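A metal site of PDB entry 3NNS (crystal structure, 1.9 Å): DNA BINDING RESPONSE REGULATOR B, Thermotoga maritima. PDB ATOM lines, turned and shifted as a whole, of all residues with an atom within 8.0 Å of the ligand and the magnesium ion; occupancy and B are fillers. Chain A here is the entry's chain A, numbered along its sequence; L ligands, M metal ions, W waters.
OD2 of Asp 9 touches the magnesium ion, at 3.9 Å.
Water W1 lies within hydrogen-bond range of the side-chain carboxylate (OD2) of Asp 9 (3.0 Å) and the side-chain amino group (NZ) of Lys 100 (3.4 Å).
The side-chain carboxylate of Asp 9 lies within salt-bridge range of the side-chain amino group of Lys 100, 2.7 Å away.
The backbone carbonyl oxygen of Val 8 sits at hydrogen-bond distance from the backbone NH of Asp 50 (2.9 Å).
The side-chain carboxylate of Asp 9 sits at hydrogen-bond distance from the backbone NH of Asp 11 (2.7 Å).
N of Gly 58 sits at hydrogen-bond distance from O of Val 51, at 2.8 Å.
N of Thr 78 sits at hydrogen-bond distance from O of Val 98, 3.0 Å away.
The backbone NH (N) of Leu 80 lies within hydrogen-bond range of the side-chain hydroxyl (OG1) of Thr 78 (3.0 Å).
The backbone NH (N) of Lys 100 is in hydrogen-bond range of the backbone carbonyl oxygen (O) of Thr 78.
The side-chain carboxylate of Asp 50 lies close to the side-chain amino group of Lys 100 (3.6 Å).
Hydrophobic or aromatic side chains that line the ligand: Val 51, Met 52 and Leu 79.
The nearest printed residue that does not touch the ligand is Asp 10 (4.2 Å).
NZ of Lys 100 sits at hydrogen-bond distance from F3 of the ligand (3.0 Å).
BE1 of the ligand is bound by OD2 of Asp 50 (1.8 Å).
A fluorine (F3) of the ligand lies within hydrogen-bond range of the backbone NH of Leu 79 (3.1 Å).
F2 of the ligand is in hydrogen-bond range of N of Val 51 (3.2 Å).
F2 of the ligand sits at hydrogen-bond distance from N of Met 52 (2.6 Å).
A fluorine (F2) of the ligand sits at hydrogen-bond distance from the side-chain hydroxyl (OG1) of Thr 78.
The magnesium ion is bound by water W2, 1.9 Å away.
Water W1 is bound to the magnesium ion.
OD2 of Asp 10 is bound to the magnesium ion, 2.0 Å away.
The side-chain carboxylate (OD1) of Asp 50 binds the magnesium ion (2.0 Å).
F1 of the ligand is bound to the magnesium ion (2.3 Å).
The magnesium ion is bound by O of Met 52 (2.4 Å).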
ATOM      1  N   VAL A   8     -12.922  -9.317 -27.764  1.00  0.00           N
ATOM      2  CA  VAL A   8     -12.330  -9.476 -29.094  1.00  0.00           C
ATOM      3  C   VAL A   8     -12.603 -10.878 -29.606  1.00  0.00           C
ATOM      4  O   VAL A   8     -12.151 -11.861 -29.027  1.00  0.00           O
ATOM      5  CB  VAL A   8     -10.804  -9.259 -29.041  1.00  0.00           C
ATOM      6  CG1 VAL A   8     -10.223  -9.178 -30.456  1.00  0.00           C
ATOM      7  CG2 VAL A   8     -10.486  -8.003 -28.249  1.00  0.00           C
ATOM      8  N   ASP A   9     -13.369 -10.956 -30.701  1.00  0.00           N
ATOM      9  CA  ASP A   9     -13.740 -12.242 -31.287  1.00  0.00           C
ATOM     10  C   ASP A   9     -14.296 -11.989 -32.678  1.00  0.00           C
ATOM     11  O   ASP A   9     -15.100 -11.072 -32.866  1.00  0.00           O
ATOM     12  CB  ASP A   9     -14.803 -12.920 -30.409  1.00  0.00           C
ATOM     13  CG  ASP A   9     -14.920 -14.419 -30.683  1.00  0.00           C
ATOM     14  OD1 ASP A   9     -14.650 -15.225 -29.754  1.00  0.00           O
ATOM     15  OD2 ASP A   9     -15.270 -14.793 -31.829  1.00  0.00           O
ATOM     16  N   ASP A  10     -13.877 -12.799 -33.652  1.00  0.00           N
ATOM     17  CA  ASP A  10     -14.356 -12.662 -35.031  1.00  0.00           C
ATOM     18  C   ASP A  10     -15.787 -13.158 -35.195  1.00  0.00           C
ATOM     19  O   ASP A  10     -16.419 -12.908 -36.223  1.00  0.00           O
ATOM     20  CB  ASP A  10     -13.433 -13.423 -35.989  1.00  0.00           C
ATOM     21  CG  ASP A  10     -13.166 -14.849 -35.556  1.00  0.00           C
ATOM     22  OD1 ASP A  10     -13.537 -15.798 -36.288  1.00  0.00           O
ATOM     23  OD2 ASP A  10     -12.592 -15.018 -34.464  1.00  0.00           O
ATOM     24  N   ASP A  11     -16.304 -13.849 -34.187  1.00  0.00           N
ATOM     25  CA  ASP A  11     -17.671 -14.373 -34.230  1.00  0.00           C
ATOM     26  C   ASP A  11     -18.643 -13.327 -33.687  1.00  0.00           C
ATOM     27  O   ASP A  11     -18.696 -13.076 -32.484  1.00  0.00           O
ATOM     28  CB  ASP A  11     -17.764 -15.673 -33.428  1.00  0.00           C
ATOM     29  CG  ASP A  11     -19.140 -16.315 -33.506  1.00  0.00           C
ATOM     30  OD1 ASP A  11     -19.282 -17.454 -33.003  1.00  0.00           O
ATOM     31  OD2 ASP A  11     -20.081 -15.704 -34.043  1.00  0.00           O
ATOM     32  N   ILE A  14     -20.725 -14.128 -30.595  1.00  0.00           N
ATOM     33  CA  ILE A  14     -20.011 -14.139 -29.317  1.00  0.00           C
ATOM     34  C   ILE A  14     -19.970 -12.705 -28.786  1.00  0.00           C
ATOM     35  O   ILE A  14     -20.209 -12.473 -27.599  1.00  0.00           O
ATOM     36  CB  ILE A  14     -18.565 -14.669 -29.474  1.00  0.00           C
ATOM     37  CG1 ILE A  14     -18.583 -16.185 -29.684  1.00  0.00           C
ATOM     38  CG2 ILE A  14     -17.729 -14.297 -28.253  1.00  0.00           C
ATOM     39  CD1 ILE A  14     -19.039 -16.976 -28.477  1.00  0.00           C
ATOM     40  N   LEU A  32     -14.051  -7.108 -33.739  1.00  0.00           N
ATOM     41  CA  LEU A  32     -14.102  -8.265 -34.614  1.00  0.00           C
ATOM     42  C   LEU A  32     -12.716  -8.787 -34.998  1.00  0.00           C
ATOM     43  O   LEU A  32     -12.584  -9.934 -35.438  1.00  0.00           O
ATOM     44  CB  LEU A  32     -14.879  -7.948 -35.905  1.00  0.00           C
ATOM     45  CG  LEU A  32     -16.415  -7.923 -35.868  1.00  0.00           C
ATOM     46  CD1 LEU A  32     -16.924  -7.566 -37.265  1.00  0.00           C
ATOM     47  CD2 LEU A  32     -16.971  -9.280 -35.439  1.00  0.00           C
ATOM     48  N   LEU A  49     -10.718 -12.285 -24.630  1.00  0.00           N
ATOM     49  CA  LEU A  49     -10.019 -12.474 -25.897  1.00  0.00           C
ATOM     50  C   LEU A  49     -10.083 -13.850 -26.552  1.00  0.00           C
ATOM     51  O   LEU A  49      -9.761 -14.873 -25.929  1.00  0.00           O
ATOM     52  CB  LEU A  49      -8.556 -12.068 -25.677  1.00  0.00           C
ATOM     53  CG  LEU A  49      -7.513 -12.209 -26.776  1.00  0.00           C
ATOM     54  CD1 LEU A  49      -7.901 -11.411 -28.012  1.00  0.00           C
ATOM     55  CD2 LEU A  49      -6.182 -11.727 -26.212  1.00  0.00           C
ATOM     56  N   ASP A  50     -10.474 -13.856 -27.820  1.00  0.00           N
ATOM     57  CA  ASP A  50     -10.574 -15.063 -28.637  1.00  0.00           C
ATOM     58  C   ASP A  50      -9.146 -15.463 -29.004  1.00  0.00           C
ATOM     59  O   ASP A  50      -8.258 -14.612 -29.051  1.00  0.00           O
ATOM     60  CB  ASP A  50     -11.382 -14.743 -29.899  1.00  0.00           C
ATOM     61  CG  ASP A  50     -11.633 -15.961 -30.770  1.00  0.00           C
ATOM     62  OD1 ASP A  50     -11.828 -15.764 -31.992  1.00  0.00           O
ATOM     63  OD2 ASP A  50     -11.640 -17.105 -30.258  1.00  0.00           O
ATOM     64  N   VAL A  51      -8.924 -16.748 -29.261  1.00  0.00           N
ATOM     65  CA  VAL A  51      -7.585 -17.191 -29.633  1.00  0.00           C
ATOM     66  C   VAL A  51      -7.410 -17.274 -31.141  1.00  0.00           C
ATOM     67  O   VAL A  51      -6.427 -16.762 -31.692  1.00  0.00           O
ATOM     68  CB  VAL A  51      -7.246 -18.560 -28.998  1.00  0.00           C
ATOM     69  CG1 VAL A  51      -5.906 -19.065 -29.526  1.00  0.00           C
ATOM     70  CG2 VAL A  51      -7.166 -18.414 -27.489  1.00  0.00           C
ATOM     71  N   MET A  52      -8.371 -17.913 -31.812  1.00  0.00           N
ATOM     72  CA  MET A  52      -8.293 -18.029 -33.263  1.00  0.00           C
ATOM     73  C   MET A  52      -8.945 -16.831 -33.956  1.00  0.00           C
ATOM     74  O   MET A  52     -10.157 -16.787 -34.158  1.00  0.00           O
ATOM     75  CB  MET A  52      -8.956 -19.331 -33.711  1.00  0.00           C
ATOM     76  CG  MET A  52      -8.435 -20.543 -32.949  1.00  0.00           C
ATOM     77  SD  MET A  52      -8.827 -22.225 -33.803  1.00  0.00           S
ATOM     78  CE  MET A  52     -10.669 -21.893 -34.309  1.00  0.00           C
ATOM     79  N   LEU A  53      -8.127 -15.847 -34.288  1.00  0.00           N
ATOM     80  CA  LEU A  53      -8.607 -14.639 -34.956  1.00  0.00           C
ATOM     81  C   LEU A  53      -8.123 -14.626 -36.402  1.00  0.00           C
ATOM     82  O   LEU A  53      -7.222 -15.385 -36.768  1.00  0.00           O
ATOM     83  CB  LEU A  53      -8.103 -13.397 -34.194  1.00  0.00           C
ATOM     84  CG  LEU A  53      -8.667 -13.247 -32.772  1.00  0.00           C
ATOM     85  CD1 LEU A  53      -7.963 -12.098 -32.046  1.00  0.00           C
ATOM     86  CD2 LEU A  53     -10.153 -12.985 -32.847  1.00  0.00           C
ATOM     87  N   PRO A  54      -8.715 -13.773 -37.243  1.00  0.00           N
ATOM     88  CA  PRO A  54      -8.337 -13.696 -38.663  1.00  0.00           C
ATOM     89  C   PRO A  54      -6.896 -13.235 -38.883  1.00  0.00           C
ATOM     90  O   PRO A  54      -6.158 -13.828 -39.678  1.00  0.00           O
ATOM     91  CB  PRO A  54      -9.341 -12.689 -39.225  1.00  0.00           C
ATOM     92  CG  PRO A  54     -10.531 -12.848 -38.342  1.00  0.00           C
ATOM     93  CD  PRO A  54      -9.890 -12.917 -36.979  1.00  0.00           C
ATOM     94  N   TYR A  56      -4.537 -11.976 -35.998  1.00  0.00           N
ATOM     95  CA  TYR A  56      -3.616 -12.335 -34.930  1.00  0.00           C
ATOM     96  C   TYR A  56      -4.113 -13.550 -34.171  1.00  0.00           C
ATOM     97  O   TYR A  56      -5.247 -13.984 -34.342  1.00  0.00           O
ATOM     98  CB  TYR A  56      -3.500 -11.201 -33.912  1.00  0.00           C
ATOM     99  CG  TYR A  56      -2.711  -9.997 -34.355  1.00  0.00           C
ATOM    100  CD1 TYR A  56      -1.377  -9.844 -33.971  1.00  0.00           C
ATOM    101  CD2 TYR A  56      -3.295  -9.001 -35.125  1.00  0.00           C
ATOM    102  CE1 TYR A  56      -0.645  -8.710 -34.351  1.00  0.00           C
ATOM    103  CE2 TYR A  56      -2.584  -7.868 -35.517  1.00  0.00           C
ATOM    104  CZ  TYR A  56      -1.255  -7.726 -35.125  1.00  0.00           C
ATOM    105  OH  TYR A  56      -0.533  -6.624 -35.492  1.00  0.00           O
ATOM    106  N   GLY A  58      -4.761 -15.005 -30.351  1.00  0.00           N
ATOM    107  CA  GLY A  58      -5.042 -14.403 -29.061  1.00  0.00           C
ATOM    108  C   GLY A  58      -3.823 -14.426 -28.159  1.00  0.00           C
ATOM    109  O   GLY A  58      -3.671 -13.587 -27.280  1.00  0.00           O
ATOM    110  N   TYR A  59      -2.946 -15.407 -28.368  1.00  0.00           N
ATOM    111  CA  TYR A  59      -1.729 -15.526 -27.567  1.00  0.00           C
ATOM    112  C   TYR A  59      -0.842 -14.313 -27.817  1.00  0.00           C
ATOM    113  O   TYR A  59      -0.264 -13.741 -26.890  1.00  0.00           O
ATOM    114  CB  TYR A  59      -0.949 -16.789 -27.912  1.00  0.00           C
ATOM    115  CG  TYR A  59      -1.704 -18.079 -27.709  1.00  0.00           C
ATOM    116  CD1 TYR A  59      -2.350 -18.350 -26.501  1.00  0.00           C
ATOM    117  CD2 TYR A  59      -1.780 -19.034 -28.718  1.00  0.00           C
ATOM    118  CE1 TYR A  59      -3.052 -19.548 -26.306  1.00  0.00           C
ATOM    119  CE2 TYR A  59      -2.468 -20.223 -28.541  1.00  0.00           C
ATOM    120  CZ  TYR A  59      -3.107 -20.473 -27.339  1.00  0.00           C
ATOM    121  OH  TYR A  59      -3.794 -21.661 -27.161  1.00  0.00           O
ATOM    122  N   LEU A  76      -8.944 -15.579 -21.829  1.00  0.00           N
ATOM    123  CA  LEU A  76      -8.993 -16.154 -23.168  1.00  0.00           C
ATOM    124  C   LEU A  76     -10.286 -16.952 -23.210  1.00  0.00           C
ATOM    125  O   LEU A  76     -10.628 -17.658 -22.264  1.00  0.00           O
ATOM    126  CB  LEU A  76      -7.785 -17.066 -23.420  1.00  0.00           C
ATOM    127  CG  LEU A  76      -6.431 -16.369 -23.640  1.00  0.00           C
ATOM    128  CD1 LEU A  76      -5.299 -17.409 -23.699  1.00  0.00           C
ATOM    129  CD2 LEU A  76      -6.480 -15.568 -24.932  1.00  0.00           C
ATOM    130  N   LEU A  77     -11.015 -16.802 -24.317  1.00  0.00           N
ATOM    131  CA  LEU A  77     -12.286 -17.476 -24.558  1.00  0.00           C
ATOM    132  C   LEU A  77     -12.130 -18.102 -25.933  1.00  0.00           C
ATOM    133  O   LEU A  77     -12.162 -17.405 -26.939  1.00  0.00           O
ATOM    134  CB  LEU A  77     -13.423 -16.453 -24.564  1.00  0.00           C
ATOM    135  CG  LEU A  77     -14.843 -17.007 -24.771  1.00  0.00           C
ATOM    136  CD1 LEU A  77     -15.185 -17.955 -23.618  1.00  0.00           C
ATOM    137  CD2 LEU A  77     -15.828 -15.851 -24.831  1.00  0.00           C
ATOM    138  N   THR A  78     -11.976 -19.426 -25.968  1.00  0.00           N
ATOM    139  CA  THR A  78     -11.733 -20.106 -27.236  1.00  0.00           C
ATOM    140  C   THR A  78     -12.281 -21.532 -27.322  1.00  0.00           C
ATOM    141  O   THR A  78     -12.550 -22.181 -26.308  1.00  0.00           O
ATOM    142  CB  THR A  78     -10.207 -20.133 -27.488  1.00  0.00           C
ATOM    143  OG1 THR A  78      -9.916 -20.917 -28.661  1.00  0.00           O
ATOM    144  CG2 THR A  78      -9.496 -20.733 -26.280  1.00  0.00           C
ATOM    145  N   LEU A  79     -12.424 -22.011 -28.556  1.00  0.00           N
ATOM    146  CA  LEU A  79     -12.915 -23.369 -28.788  1.00  0.00           C
ATOM    147  C   LEU A  79     -11.780 -24.365 -28.520  1.00  0.00           C
ATOM    148  O   LEU A  79     -12.003 -25.560 -28.453  1.00  0.00           O
ATOM    149  CB  LEU A  79     -13.431 -23.520 -30.227  1.00  0.00           C
ATOM    150  CG  LEU A  79     -12.492 -23.536 -31.431  1.00  0.00           C
ATOM    151  CD1 LEU A  79     -11.415 -22.474 -31.269  1.00  0.00           C
ATOM    152  CD2 LEU A  79     -11.855 -24.902 -31.583  1.00  0.00           C
ATOM    153  N   LEU A  80     -10.564 -23.851 -28.398  1.00  0.00           N
ATOM    154  CA  LEU A  80      -9.408 -24.697 -28.109  1.00  0.00           C
ATOM    155  C   LEU A  80      -9.554 -25.112 -26.649  1.00  0.00           C
ATOM    156  O   LEU A  80      -9.568 -24.261 -25.759  1.00  0.00           O
ATOM    157  CB  LEU A  80      -8.106 -23.904 -28.292  1.00  0.00           C
ATOM    158  CG  LEU A  80      -7.848 -23.289 -29.662  1.00  0.00           C
ATOM    159  CD1 LEU A  80      -6.574 -22.484 -29.619  1.00  0.00           C
ATOM    160  CD2 LEU A  80      -7.758 -24.377 -30.717  1.00  0.00           C
ATOM    161  N   TYR A  97      -8.682 -18.896 -18.631  1.00  0.00           N
ATOM    162  CA  TYR A  97      -8.872 -19.604 -19.884  1.00  0.00           C
ATOM    163  C   TYR A  97     -10.244 -20.264 -19.843  1.00  0.00           C
ATOM    164  O   TYR A  97     -10.450 -21.221 -19.092  1.00  0.00           O
ATOM    165  CB  TYR A  97      -7.803 -20.671 -20.056  1.00  0.00           C
ATOM    166  CG  TYR A  97      -7.637 -21.148 -21.482  1.00  0.00           C
ATOM    167  CD1 TYR A  97      -6.631 -20.630 -22.285  1.00  0.00           C
ATOM    168  CD2 TYR A  97      -8.466 -22.136 -22.011  1.00  0.00           C
ATOM    169  CE1 TYR A  97      -6.442 -21.098 -23.595  1.00  0.00           C
ATOM    170  CE2 TYR A  97      -8.287 -22.603 -23.311  1.00  0.00           C
ATOM    171  CZ  TYR A  97      -7.279 -22.080 -24.093  1.00  0.00           C
ATOM    172  OH  TYR A  97      -7.079 -22.548 -25.371  1.00  0.00           O
ATOM    173  N   VAL A  98     -11.169 -19.759 -20.646  1.00  0.00           N
ATOM    174  CA  VAL A  98     -12.513 -20.309 -20.703  1.00  0.00           C
ATOM    175  C   VAL A  98     -12.710 -20.944 -22.075  1.00  0.00           C
ATOM    176  O   VAL A  98     -12.283 -20.391 -23.097  1.00  0.00           O
ATOM    177  CB  VAL A  98     -13.569 -19.201 -20.491  1.00  0.00           C
ATOM    178  CG1 VAL A  98     -14.971 -19.766 -20.586  1.00  0.00           C
ATOM    179  CG2 VAL A  98     -13.340 -18.567 -19.117  1.00  0.00           C
ATOM    180  N   THR A  99     -13.328 -22.117 -22.114  1.00  0.00           N
ATOM    181  CA  THR A  99     -13.530 -22.797 -23.374  1.00  0.00           C
ATOM    182  C   THR A  99     -14.964 -22.723 -23.892  1.00  0.00           C
ATOM    183  O   THR A  99     -15.924 -22.678 -23.114  1.00  0.00           O
ATOM    184  CB  THR A  99     -13.126 -24.285 -23.260  1.00  0.00           C
ATOM    185  OG1 THR A  99     -13.801 -24.882 -22.142  1.00  0.00           O
ATOM    186  CG2 THR A  99     -11.622 -24.405 -23.073  1.00  0.00           C
ATOM    187  N   LYS A 100     -15.098 -22.687 -25.215  1.00  0.00           N
ATOM    188  CA  LYS A 100     -16.397 -22.650 -25.864  1.00  0.00           C
ATOM    189  C   LYS A 100     -16.745 -24.114 -26.179  1.00  0.00           C
ATOM    190  O   LYS A 100     -15.876 -24.876 -26.579  1.00  0.00           O
ATOM    191  CB  LYS A 100     -16.335 -21.870 -27.184  1.00  0.00           C
ATOM    192  CG  LYS A 100     -15.897 -20.421 -27.081  1.00  0.00           C
ATOM    193  CD  LYS A 100     -15.767 -19.840 -28.487  1.00  0.00           C
ATOM    194  CE  LYS A 100     -15.251 -18.414 -28.496  1.00  0.00           C
ATOM    195  NZ  LYS A 100     -15.164 -17.894 -29.898  1.00  0.00           N
HETATM  196 BE1  LIG L   1     -11.668 -18.746 -31.087  1.00  0.00          BE
HETATM  197  F1  LIG L   1     -11.743 -18.725 -32.572  1.00  0.00           F
HETATM  198  F2  LIG L   1     -10.324 -19.265 -30.665  1.00  0.00           F
HETATM  199  F3  LIG L   1     -12.762 -19.609 -30.534  1.00  0.00           F
HETATM  200 MG    MG M   1     -12.457 -16.794 -33.630  1.00  0.00          MG
HETATM  201  O   HOH W   1     -14.291 -17.318 -33.155  1.00  0.00           O
HETATM  202  O   HOH W   2     -12.585 -17.933 -35.172  1.00  0.00           O
